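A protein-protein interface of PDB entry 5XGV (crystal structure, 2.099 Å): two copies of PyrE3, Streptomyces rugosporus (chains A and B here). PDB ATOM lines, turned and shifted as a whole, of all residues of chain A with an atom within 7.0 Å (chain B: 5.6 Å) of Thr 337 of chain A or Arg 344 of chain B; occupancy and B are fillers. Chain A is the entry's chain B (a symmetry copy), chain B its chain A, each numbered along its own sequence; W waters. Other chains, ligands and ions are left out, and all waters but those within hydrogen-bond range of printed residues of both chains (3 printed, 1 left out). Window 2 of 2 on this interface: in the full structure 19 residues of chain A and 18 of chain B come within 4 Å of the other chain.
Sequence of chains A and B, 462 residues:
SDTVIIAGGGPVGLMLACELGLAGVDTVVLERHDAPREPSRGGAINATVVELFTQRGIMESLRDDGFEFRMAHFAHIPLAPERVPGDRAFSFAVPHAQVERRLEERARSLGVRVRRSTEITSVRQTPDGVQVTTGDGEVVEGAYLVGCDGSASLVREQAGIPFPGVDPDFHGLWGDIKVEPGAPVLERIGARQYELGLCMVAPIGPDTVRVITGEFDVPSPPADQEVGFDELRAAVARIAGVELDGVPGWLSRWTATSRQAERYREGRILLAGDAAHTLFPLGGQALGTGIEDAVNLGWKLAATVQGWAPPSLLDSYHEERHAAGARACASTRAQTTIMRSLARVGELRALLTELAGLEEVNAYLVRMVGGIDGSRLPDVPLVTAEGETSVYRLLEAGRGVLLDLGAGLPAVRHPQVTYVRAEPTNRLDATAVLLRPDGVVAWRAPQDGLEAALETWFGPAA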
ATOM      1  N   ALA A  75     -23.147  20.423  -6.190  1.00  0.00           N
ATOM      2  CA  ALA A  75     -23.852  21.309  -5.267  1.00  0.00           C
ATOM      3  C   ALA A  75     -24.271  20.574  -3.995  1.00  0.00           C
ATOM      4  O   ALA A  75     -25.379  20.759  -3.507  1.00  0.00           O
ATOM      5  CB  ALA A  75     -25.081  21.937  -5.954  1.00  0.00           C
ATOM      6  N   PHE A 216     -26.777  32.498  -0.055  1.00  0.00           N
ATOM      7  CA  PHE A 216     -27.018  33.336  -1.232  1.00  0.00           C
ATOM      8  C   PHE A 216     -28.147  34.342  -1.036  1.00  0.00           C
ATOM      9  O   PHE A 216     -28.988  34.168  -0.155  1.00  0.00           O
ATOM     10  CB  PHE A 216     -27.336  32.467  -2.448  1.00  0.00           C
ATOM     11  CG  PHE A 216     -26.117  32.033  -3.205  1.00  0.00           C
ATOM     12  CD1 PHE A 216     -25.504  32.895  -4.103  1.00  0.00           C
ATOM     13  CD2 PHE A 216     -25.573  30.777  -2.999  1.00  0.00           C
ATOM     14  CE1 PHE A 216     -24.352  32.511  -4.782  1.00  0.00           C
ATOM     15  CE2 PHE A 216     -24.427  30.384  -3.680  1.00  0.00           C
ATOM     16  CZ  PHE A 216     -23.825  31.259  -4.576  1.00  0.00           C
ATOM     17  N   ASP A 217     -28.125  35.384  -1.869  1.00  0.00           N
ATOM     18  CA  ASP A 217     -29.206  36.356  -2.038  1.00  0.00           C
ATOM     19  C   ASP A 217     -29.682  36.972  -0.724  1.00  0.00           C
ATOM     20  O   ASP A 217     -30.863  37.045  -0.411  1.00  0.00           O
ATOM     21  CB  ASP A 217     -30.353  35.709  -2.794  1.00  0.00           C
ATOM     22  CG  ASP A 217     -29.904  35.139  -4.147  1.00  0.00           C
ATOM     23  OD1 ASP A 217     -28.793  35.473  -4.620  1.00  0.00           O
ATOM     24  OD2 ASP A 217     -30.664  34.356  -4.732  1.00  0.00           O
ATOM     25  N   ALA A 330     -19.714  27.599 -16.459  1.00  0.00           N
ATOM     26  CA  ALA A 330     -21.055  27.053 -16.637  1.00  0.00           C
ATOM     27  C   ALA A 330     -21.346  25.977 -15.581  1.00  0.00           C
ATOM     28  O   ALA A 330     -22.377  26.024 -14.918  1.00  0.00           O
ATOM     29  CB  ALA A 330     -21.227  26.495 -18.037  1.00  0.00           C
ATOM     30  N   THR A 332     -19.955  25.405 -12.551  1.00  0.00           N
ATOM     31  CA  THR A 332     -20.034  25.927 -11.181  1.00  0.00           C
ATOM     32  C   THR A 332     -21.261  26.834 -10.973  1.00  0.00           C
ATOM     33  O   THR A 332     -21.841  26.852  -9.885  1.00  0.00           O
ATOM     34  CB  THR A 332     -18.739  26.694 -10.776  1.00  0.00           C
ATOM     35  OG1 THR A 332     -18.469  27.735 -11.716  1.00  0.00           O
ATOM     36  CG2 THR A 332     -17.547  25.745 -10.740  1.00  0.00           C
ATOM     37  N   ARG A 333     -21.668  27.572 -12.004  1.00  0.00           N
ATOM     38  CA  ARG A 333     -22.911  28.360 -11.900  1.00  0.00           C
ATOM     39  C   ARG A 333     -24.153  27.474 -11.875  1.00  0.00           C
ATOM     40  O   ARG A 333     -25.122  27.775 -11.177  1.00  0.00           O
ATOM     41  CB  ARG A 333     -23.037  29.357 -13.044  1.00  0.00           C
ATOM     42  CG  ARG A 333     -22.086  30.539 -12.939  1.00  0.00           C
ATOM     43  CD  ARG A 333     -22.435  31.565 -14.012  1.00  0.00           C
ATOM     44  NE  ARG A 333     -21.452  32.638 -14.092  1.00  0.00           N
ATOM     45  CZ  ARG A 333     -21.526  33.662 -14.935  1.00  0.00           C
ATOM     46  NH1 ARG A 333     -22.557  33.767 -15.769  1.00  0.00           N
ATOM     47  NH2 ARG A 333     -20.572  34.586 -14.942  1.00  0.00           N
ATOM     48  N   ALA A 334     -24.119  26.385 -12.634  1.00  0.00           N
ATOM     49  CA  ALA A 334     -25.200  25.416 -12.611  1.00  0.00           C
ATOM     50  C   ALA A 334     -25.363  24.929 -11.184  1.00  0.00           C
ATOM     51  O   ALA A 334     -26.481  24.797 -10.686  1.00  0.00           O
ATOM     52  CB  ALA A 334     -24.913  24.237 -13.558  1.00  0.00           C
ATOM     53  N   GLN A 335     -24.238  24.674 -10.529  1.00  0.00           N
ATOM     54  CA  GLN A 335     -24.281  24.278  -9.127  1.00  0.00           C
ATOM     55  C   GLN A 335     -24.794  25.374  -8.175  1.00  0.00           C
ATOM     56  O   GLN A 335     -25.711  25.126  -7.385  1.00  0.00           O
ATOM     57  CB  GLN A 335     -22.892  23.815  -8.696  1.00  0.00           C
ATOM     58  CG  GLN A 335     -22.539  22.452  -9.276  1.00  0.00           C
ATOM     59  CD  GLN A 335     -21.117  22.071  -9.012  1.00  0.00           C
ATOM     60  OE1 GLN A 335     -20.785  21.610  -7.919  1.00  0.00           O
ATOM     61  NE2 GLN A 335     -20.255  22.272 -10.005  1.00  0.00           N
ATOM     62  N   THR A 336     -24.223  26.573  -8.235  1.00  0.00           N
ATOM     63  CA  THR A 336     -24.643  27.598  -7.275  1.00  0.00           C
ATOM     64  C   THR A 336     -26.119  27.994  -7.484  1.00  0.00           C
ATOM     65  O   THR A 336     -26.781  28.423  -6.544  1.00  0.00           O
ATOM     66  CB  THR A 336     -23.749  28.858  -7.334  1.00  0.00           C
ATOM     67  OG1 THR A 336     -23.728  29.383  -8.654  1.00  0.00           O
ATOM     68  CG2 THR A 336     -22.332  28.513  -6.922  1.00  0.00           C
ATOM     69  N   THR A 337     -26.634  27.816  -8.700  1.00  0.00           N
ATOM     70  CA  THR A 337     -28.057  28.034  -8.957  1.00  0.00           C
ATOM     71  C   THR A 337     -28.943  27.275  -7.951  1.00  0.00           C
ATOM     72  O   THR A 337     -29.929  27.828  -7.480  1.00  0.00           O
ATOM     73  CB  THR A 337     -28.451  27.621 -10.395  1.00  0.00           C
ATOM     74  OG1 THR A 337     -27.759  28.451 -11.331  1.00  0.00           O
ATOM     75  CG2 THR A 337     -29.961  27.763 -10.622  1.00  0.00           C
ATOM     76  N   ILE A 338     -28.578  26.038  -7.601  1.00  0.00           N
ATOM     77  CA  ILE A 338     -29.361  25.263  -6.634  1.00  0.00           C
ATOM     78  C   ILE A 338     -28.734  25.234  -5.242  1.00  0.00           C
ATOM     79  O   ILE A 338     -28.892  24.258  -4.518  1.00  0.00           O
ATOM     80  CB  ILE A 338     -29.582  23.790  -7.085  1.00  0.00           C
ATOM     81  CG1 ILE A 338     -28.252  23.114  -7.427  1.00  0.00           C
ATOM     82  CG2 ILE A 338     -30.524  23.725  -8.282  1.00  0.00           C
ATOM     83  CD1 ILE A 338     -28.382  21.610  -7.727  1.00  0.00           C
ATOM     84  N   MET A 339     -28.036  26.306  -4.878  1.00  0.00           N
ATOM     85  CA  MET A 339     -27.507  26.463  -3.524  1.00  0.00           C
ATOM     86  C   MET A 339     -28.194  27.631  -2.826  1.00  0.00           C
ATOM     87  O   MET A 339     -27.746  28.103  -1.778  1.00  0.00           O
ATOM     88  CB  MET A 339     -25.990  26.641  -3.559  1.00  0.00           C
ATOM     89  CG  MET A 339     -25.290  25.312  -3.894  1.00  0.00           C
ATOM     90  SD  MET A 339     -23.548  25.414  -4.290  1.00  0.00           S
ATOM     91  CE  MET A 339     -22.976  26.422  -2.978  1.00  0.00           C
ATOM     92  N   ARG A 340     -29.289  28.082  -3.431  1.00  0.00           N
ATOM     93  CA  ARG A 340     -30.201  29.033  -2.816  1.00  0.00           C
ATOM     94  C   ARG A 340     -30.954  28.306  -1.675  1.00  0.00           C
ATOM     95  O   ARG A 340     -30.727  27.126  -1.458  1.00  0.00           O
ATOM     96  CB  ARG A 340     -31.183  29.607  -3.867  1.00  0.00           C
ATOM     97  CG  ARG A 340     -30.613  30.589  -4.977  1.00  0.00           C
ATOM     98  CD  ARG A 340     -29.139  30.917  -4.859  1.00  0.00           C
ATOM     99  NE  ARG A 340     -28.764  32.162  -5.547  1.00  0.00           N
ATOM    100  CZ  ARG A 340     -27.902  32.310  -6.552  1.00  0.00           C
ATOM    101  NH1 ARG A 340     -27.212  31.268  -7.033  1.00  0.00           N
ATOM    102  NH2 ARG A 340     -27.666  33.545  -7.010  1.00  0.00           N
ATOM    103  N   SER A 341     -31.855  28.981  -0.958  1.00  0.00           N
ATOM    104  CA  SER A 341     -32.633  28.329   0.101  1.00  0.00           C
ATOM    105  C   SER A 341     -33.473  27.175  -0.446  1.00  0.00           C
ATOM    106  O   SER A 341     -33.885  27.192  -1.607  1.00  0.00           O
ATOM    107  CB  SER A 341     -33.550  29.334   0.810  1.00  0.00           C
ATOM    108  OG  SER A 341     -34.556  29.766  -0.081  1.00  0.00           O
ATOM    109  N   ARG A 344     -36.708  27.593  -2.136  1.00  0.00           N
ATOM    110  CA  ARG A 344     -36.715  27.987  -3.540  1.00  0.00           C
ATOM    111  C   ARG A 344     -36.225  26.899  -4.499  1.00  0.00           C
ATOM    112  O   ARG A 344     -36.687  26.832  -5.632  1.00  0.00           O
ATOM    113  CB  ARG A 344     -35.879  29.255  -3.731  1.00  0.00           C
ATOM    114  CG  ARG A 344     -36.468  30.485  -3.044  1.00  0.00           C
ATOM    115  CD  ARG A 344     -35.472  31.638  -2.949  1.00  0.00           C
ATOM    116  NE  ARG A 344     -34.397  31.440  -1.966  1.00  0.00           N
ATOM    117  CZ  ARG A 344     -33.202  32.033  -2.026  1.00  0.00           C
ATOM    118  NH1 ARG A 344     -32.911  32.862  -3.032  1.00  0.00           N
ATOM    119  NH2 ARG A 344     -32.295  31.800  -1.084  1.00  0.00           N
ATOM    120  N   VAL A 345     -35.290  26.053  -4.065  1.00  0.00           N
ATOM    121  CA  VAL A 345     -34.718  25.068  -4.981  1.00  0.00           C
ATOM    122  C   VAL A 345     -34.756  23.612  -4.470  1.00  0.00           C
ATOM    123  O   VAL A 345     -34.196  22.709  -5.103  1.00  0.00           O
ATOM    124  CB  VAL A 345     -33.253  25.435  -5.321  1.00  0.00           C
ATOM    125  CG1 VAL A 345     -33.180  26.848  -5.889  1.00  0.00           C
ATOM    126  CG2 VAL A 345     -32.345  25.274  -4.087  1.00  0.00           C
ATOM    127  N   LEU A 348     -36.149  20.886  -6.983  1.00  0.00           N
ATOM    128  CA  LEU A 348     -35.255  20.604  -8.092  1.00  0.00           C
ATOM    129  C   LEU A 348     -34.032  19.831  -7.596  1.00  0.00           C
ATOM    130  O   LEU A 348     -33.528  18.942  -8.291  1.00  0.00           O
ATOM    131  CB  LEU A 348     -34.835  21.896  -8.805  1.00  0.00           C
ATOM    132  CG  LEU A 348     -33.899  21.775 -10.021  1.00  0.00           C
ATOM    133  CD1 LEU A 348     -34.469  20.873 -11.120  1.00  0.00           C
ATOM    134  CD2 LEU A 348     -33.629  23.143 -10.584  1.00  0.00           C
ATOM    135  N   ASP B 217     -40.478  36.425 -10.699  1.00  0.00           N
ATOM    136  CA  ASP B 217     -39.686  37.273  -9.810  1.00  0.00           C
ATOM    137  C   ASP B 217     -39.558  38.741 -10.295  1.00  0.00           C
ATOM    138  O   ASP B 217     -38.519  39.388 -10.145  1.00  0.00           O
ATOM    139  CB  ASP B 217     -38.311  36.628  -9.599  1.00  0.00           C
ATOM    140  CG  ASP B 217     -38.410  35.210  -8.991  1.00  0.00           C
ATOM    141  OD1 ASP B 217     -39.456  34.856  -8.404  1.00  0.00           O
ATOM    142  OD2 ASP B 217     -37.435  34.452  -9.103  1.00  0.00           O
ATOM    143  N   ARG B 340     -36.965  30.837 -14.334  1.00  0.00           N
ATOM    144  CA  ARG B 340     -36.434  32.180 -14.107  1.00  0.00           C
ATOM    145  C   ARG B 340     -35.621  32.634 -15.326  1.00  0.00           C
ATOM    146  O   ARG B 340     -35.478  31.891 -16.289  1.00  0.00           O
ATOM    147  CB  ARG B 340     -35.549  32.277 -12.840  1.00  0.00           C
ATOM    148  CG  ARG B 340     -36.187  31.790 -11.518  1.00  0.00           C
ATOM    149  CD  ARG B 340     -37.645  32.209 -11.461  1.00  0.00           C
ATOM    150  NE  ARG B 340     -38.282  32.254 -10.141  1.00  0.00           N
ATOM    151  CZ  ARG B 340     -39.090  31.367  -9.549  1.00  0.00           C
ATOM    152  NH1 ARG B 340     -39.394  30.169 -10.061  1.00  0.00           N
ATOM    153  NH2 ARG B 340     -39.588  31.710  -8.358  1.00  0.00           N
ATOM    154  N   SER B 341     -35.092  33.854 -15.288  1.00  0.00           N
ATOM    155  CA  SER B 341     -34.296  34.367 -16.403  1.00  0.00           C
ATOM    156  C   SER B 341     -33.046  33.518 -16.652  1.00  0.00           C
ATOM    157  O   SER B 341     -32.494  32.936 -15.727  1.00  0.00           O
ATOM    158  CB  SER B 341     -33.865  35.800 -16.150  1.00  0.00           C
ATOM    159  OG  SER B 341     -32.971  35.840 -15.060  1.00  0.00           O
ATOM    160  N   LEU B 342     -32.584  33.488 -17.896  1.00  0.00           N
ATOM    161  CA  LEU B 342     -31.419  32.679 -18.233  1.00  0.00           C
ATOM    162  C   LEU B 342     -30.156  33.266 -17.591  1.00  0.00           C
ATOM    163  O   LEU B 342     -29.164  32.574 -17.414  1.00  0.00           O
ATOM    164  CB  LEU B 342     -31.255  32.562 -19.752  1.00  0.00           C
ATOM    165  CG  LEU B 342     -32.455  31.963 -20.486  1.00  0.00           C
ATOM    166  CD1 LEU B 342     -32.132  31.735 -21.983  1.00  0.00           C
ATOM    167  CD2 LEU B 342     -32.898  30.672 -19.808  1.00  0.00           C
ATOM    168  N   ALA B 343     -30.205  34.541 -17.224  1.00  0.00           N
ATOM    169  CA  ALA B 343     -29.099  35.140 -16.486  1.00  0.00           C
ATOM    170  C   ALA B 343     -28.942  34.439 -15.132  1.00  0.00           C
ATOM    171  O   ALA B 343     -27.867  34.413 -14.546  1.00  0.00           O
ATOM    172  CB  ALA B 343     -29.320  36.643 -16.297  1.00  0.00           C
ATOM    173  N   ARG B 344     -30.018  33.855 -14.638  1.00  0.00           N
ATOM    174  CA  ARG B 344     -29.942  33.176 -13.360  1.00  0.00           C
ATOM    175  C   ARG B 344     -29.930  31.657 -13.478  1.00  0.00           C
ATOM    176  O   ARG B 344     -29.383  30.995 -12.606  1.00  0.00           O
ATOM    177  CB  ARG B 344     -31.092  33.632 -12.474  1.00  0.00           C
ATOM    178  CG  ARG B 344     -30.925  35.097 -12.028  1.00  0.00           C
ATOM    179  CD  ARG B 344     -32.111  35.538 -11.245  1.00  0.00           C
ATOM    180  NE  ARG B 344     -32.418  34.569 -10.196  1.00  0.00           N
ATOM    181  CZ  ARG B 344     -33.603  34.463  -9.605  1.00  0.00           C
ATOM    182  NH1 ARG B 344     -34.600  35.267  -9.961  1.00  0.00           N
ATOM    183  NH2 ARG B 344     -33.795  33.547  -8.663  1.00  0.00           N
ATOM    184  N   VAL B 345     -30.527  31.090 -14.530  1.00  0.00           N
ATOM    185  CA  VAL B 345     -30.654  29.634 -14.572  1.00  0.00           C
ATOM    186  C   VAL B 345     -30.200  29.004 -15.894  1.00  0.00           C
ATOM    187  O   VAL B 345     -30.364  27.802 -16.105  1.00  0.00           O
ATOM    188  CB  VAL B 345     -32.110  29.200 -14.275  1.00  0.00           C
ATOM    189  CG1 VAL B 345     -32.541  29.705 -12.896  1.00  0.00           C
ATOM    190  CG2 VAL B 345     -33.068  29.716 -15.362  1.00  0.00           C
ATOM    191  N   GLY B 346     -29.633  29.821 -16.773  1.00  0.00           N
ATOM    192  CA  GLY B 346     -29.241  29.393 -18.102  1.00  0.00           C
ATOM    193  C   GLY B 346     -28.295  28.198 -18.096  1.00  0.00           C
ATOM    194  O   GLY B 346     -28.490  27.244 -18.853  1.00  0.00           O
ATOM    195  N   GLU B 347     -27.278  28.246 -17.236  1.00  0.00           N
ATOM    196  CA  GLU B 347     -26.274  27.190 -17.185  1.00  0.00           C
ATOM    197  C   GLU B 347     -26.888  25.873 -16.705  1.00  0.00           C
ATOM    198  O   GLU B 347     -26.610  24.817 -17.261  1.00  0.00           O
ATOM    199  CB  GLU B 347     -25.093  27.599 -16.294  1.00  0.00           C
ATOM    200  CG  GLU B 347     -24.323  28.846 -16.788  1.00  0.00           C
ATOM    201  CD  GLU B 347     -24.947  30.163 -16.310  1.00  0.00           C
ATOM    202  OE1 GLU B 347     -25.957  30.130 -15.582  1.00  0.00           O
ATOM    203  OE2 GLU B 347     -24.426  31.232 -16.660  1.00  0.00           O
ATOM    204  N   LEU B 348     -27.748  25.938 -15.698  1.00  0.00           N
ATOM    205  CA  LEU B 348     -28.393  24.723 -15.199  1.00  0.00           C
ATOM    206  C   LEU B 348     -29.357  24.155 -16.232  1.00  0.00           C
ATOM    207  O   LEU B 348     -29.461  22.934 -16.379  1.00  0.00           O
ATOM    208  CB  LEU B 348     -29.131  24.982 -13.883  1.00  0.00           C
ATOM    209  CG  LEU B 348     -29.732  23.749 -13.201  1.00  0.00           C
ATOM    210  CD1 LEU B 348     -28.661  22.669 -12.957  1.00  0.00           C
ATOM    211  CD2 LEU B 348     -30.401  24.124 -11.902  1.00  0.00           C
HETATM  212  O   HOH W   1     -25.349  35.608 -16.648  1.00  0.00           O
HETATM  213  O   HOH W   2     -28.480  32.408 -10.150  1.00  0.00           O
HETATM  214  O   HOH W   3     -31.017  34.475  -7.342  1.00  0.00           O
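Water W3 lies within hydrogen-bond range of the side-chain carboxylate of Asp 217 of chain A (2.6 Å), the guanidinium group of Arg 344 of chain B (3.2 Å) and the guanidinium group of Arg 340 of chain A (3.5 Å). Water W2 lies within hydrogen-bond range of O of Arg 344 of chain B (3.0 Å) and NH2 of Arg 340 of chain A (3.4 Å). Water W1 bridges the guanidinium group (NH1) of Arg 333 of chain A and the backbone carbonyl oxygen (O) of Ala 343 of chain B.
Of the 17 printed residues of chain A, 6 touch a printed residue of chain B. Printed residues of chain A that touch a printed residue of chain B: Ala 330, Arg 333, Ala 334, Thr 337, Ile 338 and Leu 348. Hydrophobic or aromatic side chains of chain A within 4 Å of the printed part of chain B: Ala 334, Ile 338 and Leu 348. Printed residues of chain B that touch a printed residue of chain A: Arg 344, Val 345, Glu 347 and Leu 348. Hydrophobic or aromatic side chains of chain B within 4 Å of the printed part of chain A: Val 345 and Leu 348.
NH1 of Arg 344 of chain B is in salt-bridge range of OD2 of Asp 217 of chain B (3.1 Å). The side-chain hydroxyl (OG1) of Thr 336 of chain A sits at hydrogen-bond distance from the backbone carbonyl oxygen (O) of Arg 333 of chain A (3.3 Å). The side-chain hydroxyl of Thr 337 of chain A lies within hydrogen-bond range of the backbone carbonyl oxygen of Arg 333 of chain A (2.7 Å).
The backbone carbonyl oxygen of Arg 344 of chain B is in hydrogen-bond range of the side-chain hydroxyl of Thr 337 of chain A, 3.3 Å away. OE2 of Glu 347 of chain B lies within salt-bridge range of NH1 of Arg 333 of chain A, at 3.3 Å.
Leu 348 of chain B touches its own counterpart, Leu 348 of chain A. Positions printed for both chains: 217, 340, 341, 344, 345 and 348. Of the 9 pairs that touch across the chains among the printed residues, 1 has its exchanged pair printed and touching as well.
Among the printed residues, pairs that only touch across the chains: Ala 330 of chain A with Glu 347 of chain B (3.4 Å), Ala 334 of chain A with Glu 347 of chain B (3.98 Å), Ala 334 of chain A with Leu 348 of chain B (3.8 Å), Thr 337 of chain A with Val 345 of chain B (3.9 Å), Thr 337 of chain A with Leu 348 of chain B (3.9 Å), Ile 338 of chain A with Leu 348 of chain B (3.6 Å) and Leu 348 of chain A with Leu 348 of chain B (3.6 Å).
Printed residues of chain B within 4 Å of Arg 333 of chain A: Glu 347 (3.3 Å). Of the printed residues of chain B, Ala 334 of chain A touches Glu 347 (3.98 Å) and Leu 348 (3.8 Å). Of the printed residues of chain B, Leu 348 of chain A touches Leu 348. Of chain A, only Thr 337 comes within 4 Å of Arg 344 of chain B. Of the printed residues of chain A, Glu 347 of chain B touches Ala 330 (3.4 Å), Arg 333 (3.3 Å) and Ala 334 (3.98 Å). Printed residues of chain A within 4 Å of Leu 348 of chain B: Ala 334 (3.8 Å), Thr 337 (3.9 Å), Ile 338 (3.6 Å) and Leu 348 (3.6 Å). The nearest residue of chain B that does not touch Thr 337 of chain A is Glu 347 of chain B (4.9 Å). The nearest printed residue of chain B that does not touch Ile 338 of chain A is Arg 344 of chain B (7.1 Å).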
